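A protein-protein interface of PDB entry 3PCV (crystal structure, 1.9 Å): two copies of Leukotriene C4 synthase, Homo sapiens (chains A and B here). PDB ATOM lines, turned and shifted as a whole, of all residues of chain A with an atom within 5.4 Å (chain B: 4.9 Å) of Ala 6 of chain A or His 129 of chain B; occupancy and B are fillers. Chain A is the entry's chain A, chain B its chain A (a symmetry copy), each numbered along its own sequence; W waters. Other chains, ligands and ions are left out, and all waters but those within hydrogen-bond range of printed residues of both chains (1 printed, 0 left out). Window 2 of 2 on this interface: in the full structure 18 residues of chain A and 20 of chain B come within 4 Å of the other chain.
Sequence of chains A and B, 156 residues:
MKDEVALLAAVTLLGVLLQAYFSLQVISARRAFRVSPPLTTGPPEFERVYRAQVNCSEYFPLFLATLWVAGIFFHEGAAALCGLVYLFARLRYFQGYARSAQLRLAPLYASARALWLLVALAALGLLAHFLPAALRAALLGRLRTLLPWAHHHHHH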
ATOM      1  N   LYS A   2     -20.148  23.684 -29.425  1.00  0.00           N
ATOM      2  CA  LYS A   2     -18.717  23.686 -29.185  1.00  0.00           C
ATOM      3  C   LYS A   2     -17.971  24.579 -30.179  1.00  0.00           C
ATOM      4  O   LYS A   2     -17.125  25.396 -29.789  1.00  0.00           O
ATOM      5  CB  LYS A   2     -18.175  22.250 -29.243  1.00  0.00           C
ATOM      6  CG  LYS A   2     -18.732  21.340 -28.143  1.00  0.00           C
ATOM      7  CD  LYS A   2     -18.153  19.932 -28.206  1.00  0.00           C
ATOM      8  CE  LYS A   2     -18.947  19.049 -29.158  1.00  0.00           C
ATOM      9  N   ASP A   3     -18.303  24.445 -31.465  1.00  0.00           N
ATOM     10  CA  ASP A   3     -17.495  25.034 -32.535  1.00  0.00           C
ATOM     11  C   ASP A   3     -17.257  26.542 -32.457  1.00  0.00           C
ATOM     12  O   ASP A   3     -16.190  27.022 -32.828  1.00  0.00           O
ATOM     13  CB  ASP A   3     -18.071  24.669 -33.916  1.00  0.00           C
ATOM     14  N   GLU A   4     -18.253  27.302 -32.012  1.00  0.00           N
ATOM     15  CA  GLU A   4     -18.126  28.753 -32.080  1.00  0.00           C
ATOM     16  C   GLU A   4     -17.673  29.367 -30.744  1.00  0.00           C
ATOM     17  O   GLU A   4     -17.537  30.584 -30.629  1.00  0.00           O
ATOM     18  CB  GLU A   4     -19.453  29.394 -32.514  1.00  0.00           C
ATOM     19  N   VAL A   5     -17.449  28.535 -29.740  1.00  0.00           N
ATOM     20  CA  VAL A   5     -17.065  29.092 -28.445  1.00  0.00           C
ATOM     21  C   VAL A   5     -15.889  28.388 -27.802  1.00  0.00           C
ATOM     22  O   VAL A   5     -15.610  28.623 -26.629  1.00  0.00           O
ATOM     23  CB  VAL A   5     -18.248  29.098 -27.451  1.00  0.00           C
ATOM     24  CG1 VAL A   5     -19.441  29.888 -28.013  1.00  0.00           C
ATOM     25  CG2 VAL A   5     -18.650  27.666 -27.047  1.00  0.00           C
ATOM     26  N   ALA A   6     -15.202  27.511 -28.537  1.00  0.00           N
ATOM     27  CA  ALA A   6     -14.151  26.720 -27.918  1.00  0.00           C
ATOM     28  C   ALA A   6     -12.967  27.567 -27.446  1.00  0.00           C
ATOM     29  O   ALA A   6     -12.314  27.231 -26.436  1.00  0.00           O
ATOM     30  CB  ALA A   6     -13.688  25.549 -28.846  1.00  0.00           C
ATOM     31  N   LEU A   7     -12.655  28.647 -28.166  1.00  0.00           N
ATOM     32  CA  LEU A   7     -11.540  29.496 -27.737  1.00  0.00           C
ATOM     33  C   LEU A   7     -11.949  30.279 -26.477  1.00  0.00           C
ATOM     34  O   LEU A   7     -11.116  30.510 -25.599  1.00  0.00           O
ATOM     35  CB  LEU A   7     -11.166  30.535 -28.802  1.00  0.00           C
ATOM     36  CG  LEU A   7     -10.634  30.023 -30.149  1.00  0.00           C
ATOM     37  CD1 LEU A   7     -10.480  31.214 -31.104  1.00  0.00           C
ATOM     38  CD2 LEU A   7      -9.318  29.310 -29.925  1.00  0.00           C
ATOM     39  N   LEU A   8     -13.200  30.717 -26.436  1.00  0.00           N
ATOM     40  CA  LEU A   8     -13.726  31.401 -25.228  1.00  0.00           C
ATOM     41  C   LEU A   8     -13.684  30.428 -24.040  1.00  0.00           C
ATOM     42  O   LEU A   8     -13.346  30.826 -22.918  1.00  0.00           O
ATOM     43  CB  LEU A   8     -15.149  31.901 -25.432  1.00  0.00           C
ATOM     44  CG  LEU A   8     -15.348  32.789 -26.680  1.00  0.00           C
ATOM     45  CD1 LEU A   8     -16.825  33.157 -26.793  1.00  0.00           C
ATOM     46  CD2 LEU A   8     -14.449  34.062 -26.611  1.00  0.00           C
ATOM     47  N   ALA A   9     -14.045  29.165 -24.277  1.00  0.00           N
ATOM     48  CA  ALA A   9     -14.003  28.155 -23.220  1.00  0.00           C
ATOM     49  C   ALA A   9     -12.588  27.887 -22.746  1.00  0.00           C
ATOM     50  O   ALA A   9     -12.354  27.690 -21.538  1.00  0.00           O
ATOM     51  CB  ALA A   9     -14.691  26.821 -23.675  1.00  0.00           C
ATOM     52  N   ALA A  10     -11.635  27.847 -23.678  1.00  0.00           N
ATOM     53  CA  ALA A  10     -10.232  27.628 -23.329  1.00  0.00           C
ATOM     54  C   ALA A  10      -9.653  28.805 -22.495  1.00  0.00           C
ATOM     55  O   ALA A  10      -8.941  28.579 -21.502  1.00  0.00           O
ATOM     56  CB  ALA A  10      -9.372  27.417 -24.614  1.00  0.00           C
ATOM     57  N   VAL A  11      -9.951  30.040 -22.899  1.00  0.00           N
ATOM     58  CA  VAL A  11      -9.496  31.200 -22.125  1.00  0.00           C
ATOM     59  C   VAL A  11     -10.192  31.207 -20.739  1.00  0.00           C
ATOM     60  O   VAL A  11      -9.587  31.586 -19.714  1.00  0.00           O
ATOM     61  CB  VAL A  11      -9.720  32.507 -22.890  1.00  0.00           C
ATOM     62  CG1 VAL A  11      -9.431  33.765 -21.983  1.00  0.00           C
ATOM     63  CG2 VAL A  11      -8.840  32.535 -24.166  1.00  0.00           C
ATOM     64  N   GLU A  76     -14.875  35.973 -31.990  1.00  0.00           N
ATOM     65  CA  GLU A  76     -14.342  35.028 -30.996  1.00  0.00           C
ATOM     66  C   GLU A  76     -12.841  35.157 -30.779  1.00  0.00           C
ATOM     67  O   GLU A  76     -12.367  35.187 -29.631  1.00  0.00           O
ATOM     68  CB  GLU A  76     -14.703  33.571 -31.319  1.00  0.00           C
ATOM     69  CG  GLU A  76     -14.538  32.689 -30.066  1.00  0.00           C
ATOM     70  CD  GLU A  76     -14.411  31.200 -30.314  1.00  0.00           C
ATOM     71  OE1 GLU A  76     -14.245  30.752 -31.461  1.00  0.00           O
ATOM     72  OE2 GLU A  76     -14.474  30.459 -29.328  1.00  0.00           O
ATOM     73  N   PHE B  73     -18.188  20.457 -23.094  1.00  0.00           N
ATOM     74  CA  PHE B  73     -17.095  19.867 -23.848  1.00  0.00           C
ATOM     75  C   PHE B  73     -16.762  18.432 -23.482  1.00  0.00           C
ATOM     76  O   PHE B  73     -16.081  17.739 -24.245  1.00  0.00           O
ATOM     77  CB  PHE B  73     -15.857  20.765 -23.779  1.00  0.00           C
ATOM     78  CG  PHE B  73     -15.970  21.964 -24.658  1.00  0.00           C
ATOM     79  CD1 PHE B  73     -15.560  21.897 -26.001  1.00  0.00           C
ATOM     80  CD2 PHE B  73     -16.549  23.146 -24.187  1.00  0.00           C
ATOM     81  CE1 PHE B  73     -15.684  23.016 -26.847  1.00  0.00           C
ATOM     82  CE2 PHE B  73     -16.676  24.275 -25.023  1.00  0.00           C
ATOM     83  CZ  PHE B  73     -16.241  24.210 -26.364  1.00  0.00           C
ATOM     84  N   GLY B 125     -11.991  17.649 -22.291  1.00  0.00           N
ATOM     85  CA  GLY B 125     -12.956  18.050 -23.328  1.00  0.00           C
ATOM     86  C   GLY B 125     -12.374  19.029 -24.345  1.00  0.00           C
ATOM     87  O   GLY B 125     -12.588  18.895 -25.574  1.00  0.00           O
ATOM     88  N   LEU B 126     -11.641  20.031 -23.863  1.00  0.00           N
ATOM     89  CA  LEU B 126     -11.029  20.998 -24.751  1.00  0.00           C
ATOM     90  C   LEU B 126      -9.863  20.388 -25.544  1.00  0.00           C
ATOM     91  O   LEU B 126      -9.680  20.717 -26.713  1.00  0.00           O
ATOM     92  CB  LEU B 126     -10.570  22.263 -23.995  1.00  0.00           C
ATOM     93  CG  LEU B 126     -11.739  23.128 -23.505  1.00  0.00           C
ATOM     94  CD1 LEU B 126     -11.193  24.246 -22.537  1.00  0.00           C
ATOM     95  CD2 LEU B 126     -12.553  23.753 -24.676  1.00  0.00           C
ATOM     96  N   LEU B 127      -9.082  19.520 -24.910  1.00  0.00           N
ATOM     97  CA  LEU B 127      -8.006  18.835 -25.613  1.00  0.00           C
ATOM     98  C   LEU B 127      -8.582  18.002 -26.760  1.00  0.00           C
ATOM     99  O   LEU B 127      -8.069  18.050 -27.880  1.00  0.00           O
ATOM    100  CB  LEU B 127      -7.205  17.951 -24.656  1.00  0.00           C
ATOM    101  CG  LEU B 127      -6.242  18.715 -23.751  1.00  0.00           C
ATOM    102  CD1 LEU B 127      -5.671  17.808 -22.668  1.00  0.00           C
ATOM    103  CD2 LEU B 127      -5.134  19.353 -24.569  1.00  0.00           C
ATOM    104  N   ALA B 128      -9.652  17.267 -26.486  1.00  0.00           N
ATOM    105  CA  ALA B 128     -10.309  16.452 -27.506  1.00  0.00           C
ATOM    106  C   ALA B 128     -10.791  17.332 -28.650  1.00  0.00           C
ATOM    107  O   ALA B 128     -10.735  16.951 -29.835  1.00  0.00           O
ATOM    108  CB  ALA B 128     -11.458  15.664 -26.900  1.00  0.00           C
ATOM    109  N   HIS B 129     -11.248  18.531 -28.309  1.00  0.00           N
ATOM    110  CA  HIS B 129     -11.665  19.482 -29.319  1.00  0.00           C
ATOM    111  C   HIS B 129     -10.535  20.065 -30.175  1.00  0.00           C
ATOM    112  O   HIS B 129     -10.702  20.182 -31.393  1.00  0.00           O
ATOM    113  CB  HIS B 129     -12.494  20.620 -28.694  1.00  0.00           C
ATOM    114  CG  HIS B 129     -13.013  21.593 -29.703  1.00  0.00           C
ATOM    115  ND1 HIS B 129     -14.250  21.460 -30.294  1.00  0.00           N
ATOM    116  CD2 HIS B 129     -12.453  22.698 -30.244  1.00  0.00           C
ATOM    117  CE1 HIS B 129     -14.436  22.452 -31.148  1.00  0.00           C
ATOM    118  NE2 HIS B 129     -13.361  23.215 -31.137  1.00  0.00           N
ATOM    119  N   PHE B 130      -9.419  20.462 -29.568  1.00  0.00           N
ATOM    120  CA  PHE B 130      -8.380  21.211 -30.276  1.00  0.00           C
ATOM    121  C   PHE B 130      -7.228  20.343 -30.799  1.00  0.00           C
ATOM    122  O   PHE B 130      -6.670  20.632 -31.856  1.00  0.00           O
ATOM    123  CB  PHE B 130      -7.756  22.309 -29.411  1.00  0.00           C
ATOM    124  CG  PHE B 130      -8.630  23.516 -29.234  1.00  0.00           C
ATOM    125  CD1 PHE B 130      -8.828  24.411 -30.284  1.00  0.00           C
ATOM    126  CD2 PHE B 130      -9.256  23.761 -28.011  1.00  0.00           C
ATOM    127  CE1 PHE B 130      -9.641  25.531 -30.121  1.00  0.00           C
ATOM    128  CE2 PHE B 130     -10.087  24.871 -27.851  1.00  0.00           C
ATOM    129  CZ  PHE B 130     -10.271  25.757 -28.899  1.00  0.00           C
ATOM    130  N   LEU B 131      -6.840  19.336 -30.022  1.00  0.00           N
ATOM    131  CA  LEU B 131      -5.601  18.600 -30.290  1.00  0.00           C
ATOM    132  C   LEU B 131      -5.571  18.020 -31.711  1.00  0.00           C
ATOM    133  O   LEU B 131      -4.545  18.075 -32.379  1.00  0.00           O
ATOM    134  CB  LEU B 131      -5.406  17.487 -29.263  1.00  0.00           C
ATOM    135  CG  LEU B 131      -4.036  16.809 -29.243  1.00  0.00           C
ATOM    136  CD1 LEU B 131      -2.924  17.855 -29.119  1.00  0.00           C
ATOM    137  CD2 LEU B 131      -3.979  15.794 -28.103  1.00  0.00           C
ATOM    138  N   PRO B 132      -6.701  17.461 -32.167  1.00  0.00           N
ATOM    139  CA  PRO B 132      -6.807  16.892 -33.518  1.00  0.00           C
ATOM    140  C   PRO B 132      -6.517  17.874 -34.639  1.00  0.00           C
ATOM    141  O   PRO B 132      -5.602  17.629 -35.430  1.00  0.00           O
ATOM    142  CB  PRO B 132      -8.266  16.434 -33.590  1.00  0.00           C
ATOM    143  CG  PRO B 132      -8.584  16.057 -32.179  1.00  0.00           C
ATOM    144  CD  PRO B 132      -7.846  17.087 -31.322  1.00  0.00           C
HETATM  145  O   HOH W   1     -13.022  25.721 -32.604  1.00  0.00           O
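No position is printed for both chains.
Among the printed residues, merely in contact across the chains: Ala 6 of chain A with His 129 of chain B (3.3 Å), Ala 6 of chain A with Phe 130 of chain B (3.4 Å), Ala 9 of chain A with Phe 73 of chain B (3.5 Å), Lys 2 of chain A with Phe 73 of chain B (3.5 Å), Ala 10 of chain A with Leu 126 of chain B (3.6 Å), Ala 6 of chain A with Phe 73 of chain B (3.6 Å), Ala 9 of chain A with Leu 126 of chain B (3.8 Å), Leu 7 of chain A with Phe 130 of chain B (3.8 Å) and Ala 6 of chain A with Leu 126 of chain B (3.9 Å).
Water W1 lies within hydrogen-bond range of a ring nitrogen (NE2) of His 129 of chain B and the backbone carbonyl oxygen of Asp 3 of chain A.
OE2 of Glu 76 of chain A is in hydrogen-bond range of N of Ala 6 of chain A, 3.1 Å away. The backbone NH (N) of Leu 7 of chain A is in hydrogen-bond range of the side-chain carboxylate (OE2) of Glu 76 of chain A, at 2.8 Å.
Of chain B, only Phe 73 (3.6 Å), Leu 126 (3.9 Å), His 129 (3.3 Å) and Phe 130 (3.4 Å) come within 4 Å of Ala 6 of chain A. Of chain A, only Ala 6 comes within 4 Å of His 129 of chain B. Of the printed residues of chain B, Ala 9 of chain A touches Phe 73 (3.5 Å) and Leu 126 (3.8 Å). Of the printed residues of chain B, Ala 10 of chain A touches Leu 126 (3.6 Å). Of the printed residues of chain A, Leu 126 of chain B touches Ala 6 (3.9 Å), Ala 9 (3.8 Å) and Ala 10 (3.6 Å). Leu 131 of chain B touches none of the printed residues of chain A. The nearest residue of chain A that does not touch His 129 of chain B is Lys 2 of chain A (4.1 Å).
Printed residues of chain B that touch a printed residue of chain A: Phe 73, Leu 126, His 129 and Phe 130. Among the printed residues, 9 pairs touch across the chains. Among the printed residues, no Asp or Glu carboxylate lies within 4 Å of a Lys or Arg side-chain nitrogen of the other chain.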
